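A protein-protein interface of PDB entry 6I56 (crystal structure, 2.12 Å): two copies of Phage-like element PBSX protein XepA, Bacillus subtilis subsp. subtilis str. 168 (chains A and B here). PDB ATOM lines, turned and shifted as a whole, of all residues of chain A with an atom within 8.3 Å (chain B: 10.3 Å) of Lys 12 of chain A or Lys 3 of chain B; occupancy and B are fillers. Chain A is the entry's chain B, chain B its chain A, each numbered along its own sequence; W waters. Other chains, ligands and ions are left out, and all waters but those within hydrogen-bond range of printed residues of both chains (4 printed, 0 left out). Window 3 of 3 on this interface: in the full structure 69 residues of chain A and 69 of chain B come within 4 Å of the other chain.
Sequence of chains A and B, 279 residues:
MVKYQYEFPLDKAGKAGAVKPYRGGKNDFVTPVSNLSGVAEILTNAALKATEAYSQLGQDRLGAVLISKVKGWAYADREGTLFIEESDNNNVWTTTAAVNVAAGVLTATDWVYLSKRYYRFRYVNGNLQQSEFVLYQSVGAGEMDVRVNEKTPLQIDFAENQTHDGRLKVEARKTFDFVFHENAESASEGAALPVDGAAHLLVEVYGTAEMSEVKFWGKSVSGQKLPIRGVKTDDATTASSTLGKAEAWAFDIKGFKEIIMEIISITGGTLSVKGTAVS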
ATOM      1  N   PHE A   8     -22.990 -10.418 -21.771  1.00  0.00           N
ATOM      2  CA  PHE A   8     -22.507  -9.873 -20.484  1.00  0.00           C
ATOM      3  C   PHE A   8     -23.269  -8.585 -20.226  1.00  0.00           C
ATOM      4  O   PHE A   8     -23.420  -7.740 -21.122  1.00  0.00           O
ATOM      5  CB  PHE A   8     -21.001  -9.647 -20.476  1.00  0.00           C
ATOM      6  CG  PHE A   8     -20.183 -10.905 -20.644  1.00  0.00           C
ATOM      7  CD1 PHE A   8     -20.481 -12.045 -19.937  1.00  0.00           C
ATOM      8  CD2 PHE A   8     -19.129 -10.965 -21.543  1.00  0.00           C
ATOM      9  CE1 PHE A   8     -19.744 -13.204 -20.111  1.00  0.00           C
ATOM     10  CE2 PHE A   8     -18.395 -12.125 -21.723  1.00  0.00           C
ATOM     11  CZ  PHE A   8     -18.692 -13.237 -20.998  1.00  0.00           C
ATOM     12  N   PRO A   9     -23.830  -8.422 -19.018  1.00  0.00           N
ATOM     13  CA  PRO A   9     -24.455  -7.153 -18.644  1.00  0.00           C
ATOM     14  C   PRO A   9     -23.413  -6.052 -18.440  1.00  0.00           C
ATOM     15  O   PRO A   9     -22.243  -6.355 -18.316  1.00  0.00           O
ATOM     16  CB  PRO A   9     -25.158  -7.495 -17.325  1.00  0.00           C
ATOM     17  CG  PRO A   9     -24.285  -8.584 -16.759  1.00  0.00           C
ATOM     18  CD  PRO A   9     -23.921  -9.429 -17.970  1.00  0.00           C
ATOM     19  N   LEU A  10     -23.897  -4.828 -18.363  1.00  0.00           N
ATOM     20  CA  LEU A  10     -23.110  -3.587 -18.187  1.00  0.00           C
ATOM     21  C   LEU A  10     -23.375  -3.030 -16.791  1.00  0.00           C
ATOM     22  O   LEU A  10     -24.514  -3.105 -16.306  1.00  0.00           O
ATOM     23  CB  LEU A  10     -23.496  -2.551 -19.252  1.00  0.00           C
ATOM     24  CG  LEU A  10     -23.370  -2.954 -20.720  1.00  0.00           C
ATOM     25  CD1 LEU A  10     -23.563  -1.754 -21.632  1.00  0.00           C
ATOM     26  CD2 LEU A  10     -22.041  -3.589 -20.992  1.00  0.00           C
ATOM     27  N   ASP A  11     -22.352  -2.474 -16.159  1.00  0.00           N
ATOM     28  CA  ASP A  11     -22.515  -1.777 -14.861  1.00  0.00           C
ATOM     29  C   ASP A  11     -23.043  -0.382 -15.157  1.00  0.00           C
ATOM     30  O   ASP A  11     -23.293  -0.064 -16.338  1.00  0.00           O
ATOM     31  CB  ASP A  11     -21.223  -1.782 -14.032  1.00  0.00           C
ATOM     32  CG  ASP A  11     -20.223  -0.688 -14.350  1.00  0.00           C
ATOM     33  OD1 ASP A  11     -20.255  -0.137 -15.454  1.00  0.00           O
ATOM     34  OD2 ASP A  11     -19.390  -0.439 -13.477  1.00  0.00           O
ATOM     35  N   LYS A  12     -23.171   0.436 -14.119  1.00  0.00           N
ATOM     36  CA  LYS A  12     -23.814   1.773 -14.225  1.00  0.00           C
ATOM     37  C   LYS A  12     -22.968   2.632 -15.160  1.00  0.00           C
ATOM     38  O   LYS A  12     -23.526   3.430 -15.837  1.00  0.00           O
ATOM     39  CB  LYS A  12     -24.007   2.349 -12.825  1.00  0.00           C
ATOM     40  CG  LYS A  12     -24.537   3.770 -12.791  1.00  0.00           C
ATOM     41  CD  LYS A  12     -24.650   4.277 -11.385  1.00  0.00           C
ATOM     42  CE  LYS A  12     -24.991   5.738 -11.275  1.00  0.00           C
ATOM     43  NZ  LYS A  12     -24.810   6.098  -9.850  1.00  0.00           N
ATOM     44  N   ALA A  13     -21.649   2.434 -15.201  1.00  0.00           N
ATOM     45  CA  ALA A  13     -20.702   3.205 -16.059  1.00  0.00           C
ATOM     46  C   ALA A  13     -20.500   2.540 -17.432  1.00  0.00           C
ATOM     47  O   ALA A  13     -19.645   2.979 -18.164  1.00  0.00           O
ATOM     48  CB  ALA A  13     -19.396   3.362 -15.307  1.00  0.00           C
ATOM     49  N   GLY A  14     -21.290   1.534 -17.781  1.00  0.00           N
ATOM     50  CA  GLY A  14     -21.271   0.911 -19.123  1.00  0.00           C
ATOM     51  C   GLY A  14     -20.220  -0.174 -19.261  1.00  0.00           C
ATOM     52  O   GLY A  14     -19.987  -0.587 -20.382  1.00  0.00           O
ATOM     53  N   LYS A  15     -19.642  -0.678 -18.165  1.00  0.00           N
ATOM     54  CA  LYS A  15     -18.563  -1.702 -18.222  1.00  0.00           C
ATOM     55  C   LYS A  15     -19.137  -3.125 -18.172  1.00  0.00           C
ATOM     56  O   LYS A  15     -19.889  -3.454 -17.241  1.00  0.00           O
ATOM     57  CB  LYS A  15     -17.594  -1.465 -17.059  1.00  0.00           C
ATOM     58  CG  LYS A  15     -16.737  -0.215 -17.213  1.00  0.00           C
ATOM     59  CD  LYS A  15     -16.313   0.389 -15.905  1.00  0.00           C
ATOM     60  CE  LYS A  15     -15.424   1.578 -16.146  1.00  0.00           C
ATOM     61  NZ  LYS A  15     -15.604   2.520 -15.042  1.00  0.00           N
ATOM     62  N   ALA A  16     -18.763  -3.944 -19.143  1.00  0.00           N
ATOM     63  CA  ALA A  16     -19.154  -5.362 -19.250  1.00  0.00           C
ATOM     64  C   ALA A  16     -18.445  -6.188 -18.192  1.00  0.00           C
ATOM     65  O   ALA A  16     -17.289  -5.866 -17.817  1.00  0.00           O
ATOM     66  CB  ALA A  16     -18.827  -5.907 -20.624  1.00  0.00           C
ATOM     67  N   PRO A  21     -26.555  -9.343 -11.549  1.00  0.00           N
ATOM     68  CA  PRO A  21     -26.938  -8.348 -10.552  1.00  0.00           C
ATOM     69  C   PRO A  21     -27.649  -9.062  -9.400  1.00  0.00           C
ATOM     70  O   PRO A  21     -28.164 -10.161  -9.625  1.00  0.00           O
ATOM     71  CB  PRO A  21     -27.873  -7.429 -11.342  1.00  0.00           C
ATOM     72  CG  PRO A  21     -28.559  -8.389 -12.312  1.00  0.00           C
ATOM     73  CD  PRO A  21     -27.464  -9.360 -12.707  1.00  0.00           C
ATOM     74  N   LYS A  26     -30.928  -4.368  -7.508  1.00  0.00           N
ATOM     75  CA  LYS A  26     -29.973  -4.895  -8.535  1.00  0.00           C
ATOM     76  C   LYS A  26     -28.767  -3.968  -8.613  1.00  0.00           C
ATOM     77  O   LYS A  26     -28.277  -3.680  -9.706  1.00  0.00           O
ATOM     78  CB  LYS A  26     -30.675  -5.035  -9.876  1.00  0.00           C
ATOM     79  CG  LYS A  26     -31.961  -5.832  -9.784  1.00  0.00           C
ATOM     80  CD  LYS A  26     -31.897  -7.091 -10.511  1.00  0.00           C
ATOM     81  CE  LYS A  26     -32.518  -6.926 -11.885  1.00  0.00           C
ATOM     82  NZ  LYS A  26     -33.926  -7.384 -11.831  1.00  0.00           N
ATOM     83  N   ASN A  27     -28.291  -3.546  -7.455  1.00  0.00           N
ATOM     84  CA  ASN A  27     -27.197  -2.552  -7.301  1.00  0.00           C
ATOM     85  C   ASN A  27     -25.964  -3.255  -6.766  1.00  0.00           C
ATOM     86  O   ASN A  27     -25.022  -2.568  -6.391  1.00  0.00           O
ATOM     87  CB  ASN A  27     -27.632  -1.364  -6.440  1.00  0.00           C
ATOM     88  CG  ASN A  27     -28.026  -1.756  -5.037  1.00  0.00           C
ATOM     89  OD1 ASN A  27     -28.309  -2.899  -4.710  1.00  0.00           O
ATOM     90  ND2 ASN A  27     -28.048  -0.772  -4.169  1.00  0.00           N
ATOM     91  N   MET B   1     -26.276  -4.228 -24.258  1.00  0.00           N
ATOM     92  CA  MET B   1     -27.738  -4.035 -24.498  1.00  0.00           C
ATOM     93  C   MET B   1     -28.441  -3.732 -23.157  1.00  0.00           C
ATOM     94  O   MET B   1     -29.539  -3.138 -23.221  1.00  0.00           O
ATOM     95  CB  MET B   1     -28.360  -5.276 -25.164  1.00  0.00           C
ATOM     96  N   VAL B   2     -27.805  -4.044 -22.004  1.00  0.00           N
ATOM     97  CA  VAL B   2     -28.443  -4.290 -20.657  1.00  0.00           C
ATOM     98  C   VAL B   2     -27.604  -3.624 -19.533  1.00  0.00           C
ATOM     99  O   VAL B   2     -26.544  -4.173 -19.145  1.00  0.00           O
ATOM    100  CB  VAL B   2     -28.623  -5.810 -20.400  1.00  0.00           C
ATOM    101  CG1 VAL B   2     -28.825  -6.149 -18.925  1.00  0.00           C
ATOM    102  CG2 VAL B   2     -29.735  -6.432 -21.242  1.00  0.00           C
ATOM    103  N   LYS B   3     -28.065  -2.497 -18.991  1.00  0.00           N
ATOM    104  CA  LYS B   3     -27.281  -1.652 -18.049  1.00  0.00           C
ATOM    105  C   LYS B   3     -27.965  -1.621 -16.680  1.00  0.00           C
ATOM    106  O   LYS B   3     -29.116  -1.184 -16.607  1.00  0.00           O
ATOM    107  CB  LYS B   3     -27.107  -0.247 -18.624  1.00  0.00           C
ATOM    108  CG  LYS B   3     -26.100   0.602 -17.863  1.00  0.00           C
ATOM    109  CD  LYS B   3     -25.904   1.961 -18.476  1.00  0.00           C
ATOM    110  CE  LYS B   3     -25.675   1.862 -19.966  1.00  0.00           C
ATOM    111  NZ  LYS B   3     -25.031   3.086 -20.469  1.00  0.00           N
ATOM    112  N   TYR B   4     -27.285  -2.102 -15.633  1.00  0.00           N
ATOM    113  CA  TYR B   4     -27.814  -2.180 -14.247  1.00  0.00           C
ATOM    114  C   TYR B   4     -27.253  -1.059 -13.374  1.00  0.00           C
ATOM    115  O   TYR B   4     -26.403  -0.296 -13.821  1.00  0.00           O
ATOM    116  CB  TYR B   4     -27.500  -3.551 -13.645  1.00  0.00           C
ATOM    117  CG  TYR B   4     -28.269  -4.651 -14.317  1.00  0.00           C
ATOM    118  CD1 TYR B   4     -29.625  -4.822 -14.067  1.00  0.00           C
ATOM    119  CD2 TYR B   4     -27.677  -5.444 -15.286  1.00  0.00           C
ATOM    120  CE1 TYR B   4     -30.351  -5.799 -14.719  1.00  0.00           C
ATOM    121  CE2 TYR B   4     -28.378  -6.461 -15.902  1.00  0.00           C
ATOM    122  CZ  TYR B   4     -29.726  -6.618 -15.641  1.00  0.00           C
ATOM    123  OH  TYR B   4     -30.418  -7.597 -16.289  1.00  0.00           O
ATOM    124  N   GLN B   5     -27.745  -0.988 -12.136  1.00  0.00           N
ATOM    125  CA  GLN B   5     -27.425   0.074 -11.164  1.00  0.00           C
ATOM    126  C   GLN B   5     -26.180  -0.295 -10.366  1.00  0.00           C
ATOM    127  O   GLN B   5     -25.616   0.615  -9.720  1.00  0.00           O
ATOM    128  CB  GLN B   5     -28.645   0.388 -10.284  1.00  0.00           C
ATOM    129  CG  GLN B   5     -29.699   1.246 -10.952  1.00  0.00           C
ATOM    130  CD  GLN B   5     -29.054   2.494 -11.502  1.00  0.00           C
ATOM    131  OE1 GLN B   5     -28.880   2.628 -12.713  1.00  0.00           O
ATOM    132  NE2 GLN B   5     -28.609   3.370 -10.613  1.00  0.00           N
ATOM    133  N   TYR B   6     -25.712  -1.545 -10.379  1.00  0.00           N
ATOM    134  CA  TYR B   6     -24.416  -1.886  -9.720  1.00  0.00           C
ATOM    135  C   TYR B   6     -23.292  -1.109 -10.424  1.00  0.00           C
ATOM    136  O   TYR B   6     -23.414  -0.766 -11.605  1.00  0.00           O
ATOM    137  CB  TYR B   6     -24.210  -3.404  -9.659  1.00  0.00           C
ATOM    138  CG  TYR B   6     -23.966  -4.109 -10.975  1.00  0.00           C
ATOM    139  CD1 TYR B   6     -22.756  -4.051 -11.633  1.00  0.00           C
ATOM    140  CD2 TYR B   6     -24.954  -4.885 -11.541  1.00  0.00           C
ATOM    141  CE1 TYR B   6     -22.549  -4.690 -12.845  1.00  0.00           C
ATOM    142  CE2 TYR B   6     -24.762  -5.553 -12.738  1.00  0.00           C
ATOM    143  CZ  TYR B   6     -23.540  -5.473 -13.388  1.00  0.00           C
ATOM    144  OH  TYR B   6     -23.320  -6.054 -14.608  1.00  0.00           O
ATOM    145  N   GLU B   7     -22.220  -0.800  -9.707  1.00  0.00           N
ATOM    146  CA  GLU B   7     -21.069  -0.064 -10.286  1.00  0.00           C
ATOM    147  C   GLU B   7     -19.769  -0.740  -9.837  1.00  0.00           C
ATOM    148  O   GLU B   7     -19.588  -0.915  -8.662  1.00  0.00           O
ATOM    149  CB  GLU B   7     -21.066   1.409  -9.884  1.00  0.00           C
ATOM    150  CG  GLU B   7     -20.099   2.214 -10.750  1.00  0.00           C
ATOM    151  CD  GLU B   7     -20.185   3.732 -10.664  1.00  0.00           C
ATOM    152  OE1 GLU B   7     -21.007   4.302 -11.380  1.00  0.00           O
ATOM    153  OE2 GLU B   7     -19.425   4.335  -9.874  1.00  0.00           O
ATOM    154  N   PHE B   8     -18.895  -1.091 -10.766  1.00  0.00           N
ATOM    155  CA  PHE B   8     -17.593  -1.679 -10.410  1.00  0.00           C
ATOM    156  C   PHE B   8     -16.766  -0.586  -9.761  1.00  0.00           C
ATOM    157  O   PHE B   8     -16.685   0.525 -10.250  1.00  0.00           O
ATOM    158  CB  PHE B   8     -16.878  -2.310 -11.610  1.00  0.00           C
ATOM    159  CG  PHE B   8     -17.625  -3.448 -12.267  1.00  0.00           C
ATOM    160  CD1 PHE B   8     -18.218  -4.445 -11.511  1.00  0.00           C
ATOM    161  CD2 PHE B   8     -17.682  -3.538 -13.628  1.00  0.00           C
ATOM    162  CE1 PHE B   8     -18.897  -5.482 -12.111  1.00  0.00           C
ATOM    163  CE2 PHE B   8     -18.328  -4.599 -14.257  1.00  0.00           C
ATOM    164  CZ  PHE B   8     -18.958  -5.555 -13.495  1.00  0.00           C
ATOM    165  N   PRO B   9     -16.152  -0.878  -8.600  1.00  0.00           N
ATOM    166  CA  PRO B   9     -15.196   0.034  -8.001  1.00  0.00           C
ATOM    167  C   PRO B   9     -13.892   0.092  -8.789  1.00  0.00           C
ATOM    168  O   PRO B   9     -13.647  -0.801  -9.617  1.00  0.00           O
ATOM    169  CB  PRO B   9     -14.955  -0.596  -6.615  1.00  0.00           C
ATOM    170  CG  PRO B   9     -15.156  -2.062  -6.874  1.00  0.00           C
ATOM    171  CD  PRO B   9     -16.338  -2.115  -7.817  1.00  0.00           C
ATOM    172  N   ALA B  16     -11.328  -0.488 -13.192  1.00  0.00           N
ATOM    173  CA  ALA B  16     -12.547  -1.200 -12.766  1.00  0.00           C
ATOM    174  C   ALA B  16     -12.238  -2.689 -12.633  1.00  0.00           C
ATOM    175  O   ALA B  16     -11.370  -3.218 -13.374  1.00  0.00           O
ATOM    176  CB  ALA B  16     -13.645  -0.980 -13.766  1.00  0.00           C
HETATM  177  O   HOH W   1     -21.046  -5.691 -15.736  1.00  0.00           O
HETATM  178  O   HOH W   2     -22.411  -1.492  -6.598  1.00  0.00           O
HETATM  179  O   HOH W   3     -25.534  -6.382 -22.007  1.00  0.00           O
HETATM  180  O   HOH W   4     -17.455   0.966 -12.882  1.00  0.00           O
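The side-chain carboxylate (OD1) of Asp 11 of chain A sits at hydrogen-bond distance from the backbone NH (N) of Ala 13 of chain A (2.9 Å).
The side-chain carboxylate (OD1) of Asp 11 of chain A lies within hydrogen-bond range of the backbone NH (N) of Gly 14 of chain A (3.0 Å).
The backbone NH (N) of Lys 15 of chain A is in hydrogen-bond range of the side-chain carboxylate (OD1) of Asp 11 of chain A (2.8 Å).
Ala 16 of chain A touches Phe 8 of chain B, but with the chains exchanged Phe 8 of chain A does not touch Ala 16 of chain B (13.2 Å).
3 positions are printed for both chains.
Of the 27 pairs that touch across the chains among the printed residues, none has its exchanged pair printed and touching as well.
Among the printed residues, pairs that only touch across the chains: Asp 11 of chain A with Lys 3 of chain B (3.3 Å), Asn 27 of chain A with Tyr 6 of chain B (3.4 Å), Asp 11 of chain A with Tyr 6 of chain B (3.4 Å), Pro 9 of chain A with Tyr 6 of chain B (3.5 Å), Lys 15 of chain A with Phe 8 of chain B (3.6 Å), Leu 10 of chain A with Lys 3 of chain B (3.6 Å), Leu 10 of chain A with Tyr 6 of chain B (3.6 Å), Asp 11 of chain A with Tyr 4 of chain B (3.6 Å), Asp 11 of chain A with Glu 7 of chain B (3.6 Å), Lys 12 of chain A with Glu 7 of chain B (3.6 Å), Lys 26 of chain A with Gln 5 of chain B (3.7 Å), Pro 9 of chain A with Tyr 4 of chain B (3.7 Å), Pro 9 of chain A with Val 2 of chain B (3.7 Å), Lys 15 of chain A with Ala 16 of chain B (3.7 Å), Lys 26 of chain A with Tyr 4 of chain B (3.7 Å), Lys 12 of chain A with Lys 3 of chain B (3.8 Å), Pro 21 of chain A with Tyr 6 of chain B (3.9 Å), Lys 12 of chain A with Gln 5 of chain B (3.9 Å), Ala 16 of chain A with Phe 8 of chain B (3.9 Å), Asn 27 of chain A with Gln 5 of chain B (3.9 Å) and Pro 21 of chain A with Tyr 4 of chain B (3.9 Å).
Water W4 lies within hydrogen-bond range of the side-chain carboxylate of Asp 11 of chain A, the backbone carbonyl oxygen of Phe 8 of chain B and the side-chain amino group of Lys 15 of chain A.
Water W1 lies within hydrogen-bond range of OH of Tyr 6 of chain B (2.6 Å), O of Pro 9 of chain A (2.9 Å), O of Lys 15 of chain A (2.9 Å) and N of Asp 11 of chain A (3.5 Å).
Water W3 lies within hydrogen-bond range of O of Phe 8 of chain A, N of Met 1 of chain B and N of Val 2 of chain B.
Water W2 bridges the backbone carbonyl oxygen (O) of Asn 27 of chain A (2.8 Å) and the backbone NH (N) of Glu 7 of chain B (3.2 Å).
The backbone carbonyl oxygen of Val 2 of chain B lies within hydrogen-bond range of the backbone NH of Leu 10 of chain A, 2.8 Å away.
O of Leu 10 of chain A lies within hydrogen-bond range of N of Tyr 4 of chain B (3.0 Å).
The backbone NH of Lys 12 of chain A is in hydrogen-bond range of the backbone carbonyl oxygen of Tyr 4 of chain B, at 3.3 Å.
O of Tyr 6 of chain B is in hydrogen-bond range of N of Lys 12 of chain A (2.8 Å).
N of Tyr 6 of chain B is in hydrogen-bond range of O of Lys 26 of chain A (3.4 Å).
OD2 of Asp 11 of chain A sits at hydrogen-bond distance from N of Phe 8 of chain B (2.8 Å).
Lys 12 of chain A touches five residues of chain B.
Ala 13 of chain A touches none of the printed residues of chain B.
No residue of chain B comes within 4 Å of Gly 14 of chain A.
Lys 3 of chain B touches three residues of chain A.
Of the printed residues of chain A, Tyr 4 of chain B touches Pro 9, Leu 10, Asp 11, Lys 12, Pro 21 and Lys 26.
Of the printed residues of chain A, Ala 16 of chain B touches Lys 15 (3.7 Å).
The nearest printed residue of chain A that does not touch Tyr 6 of chain B is Lys 15 of chain A (5.0 Å).
Printed residues of chain A that touch a printed residue of chain B: Pro 9, Leu 10, Asp 11, Lys 12, Lys 15, Ala 16, Pro 21, Lys 26 and Asn 27.
Hydrophobic or aromatic side chains of chain A within 4 Å of the printed part of chain B: Pro 9, Leu 10 and Pro 21.
Hydrophobic or aromatic side chains of chain B that line the printed part of chain A: Tyr 4, Tyr 6, Phe 8 and Ala 16.
Among the printed residues, 27 pairs touch across the chains.
Among the printed residues, no Asp or Glu carboxylate lies within 4 Å of a Lys or Arg side-chain nitrogen of the other chain.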
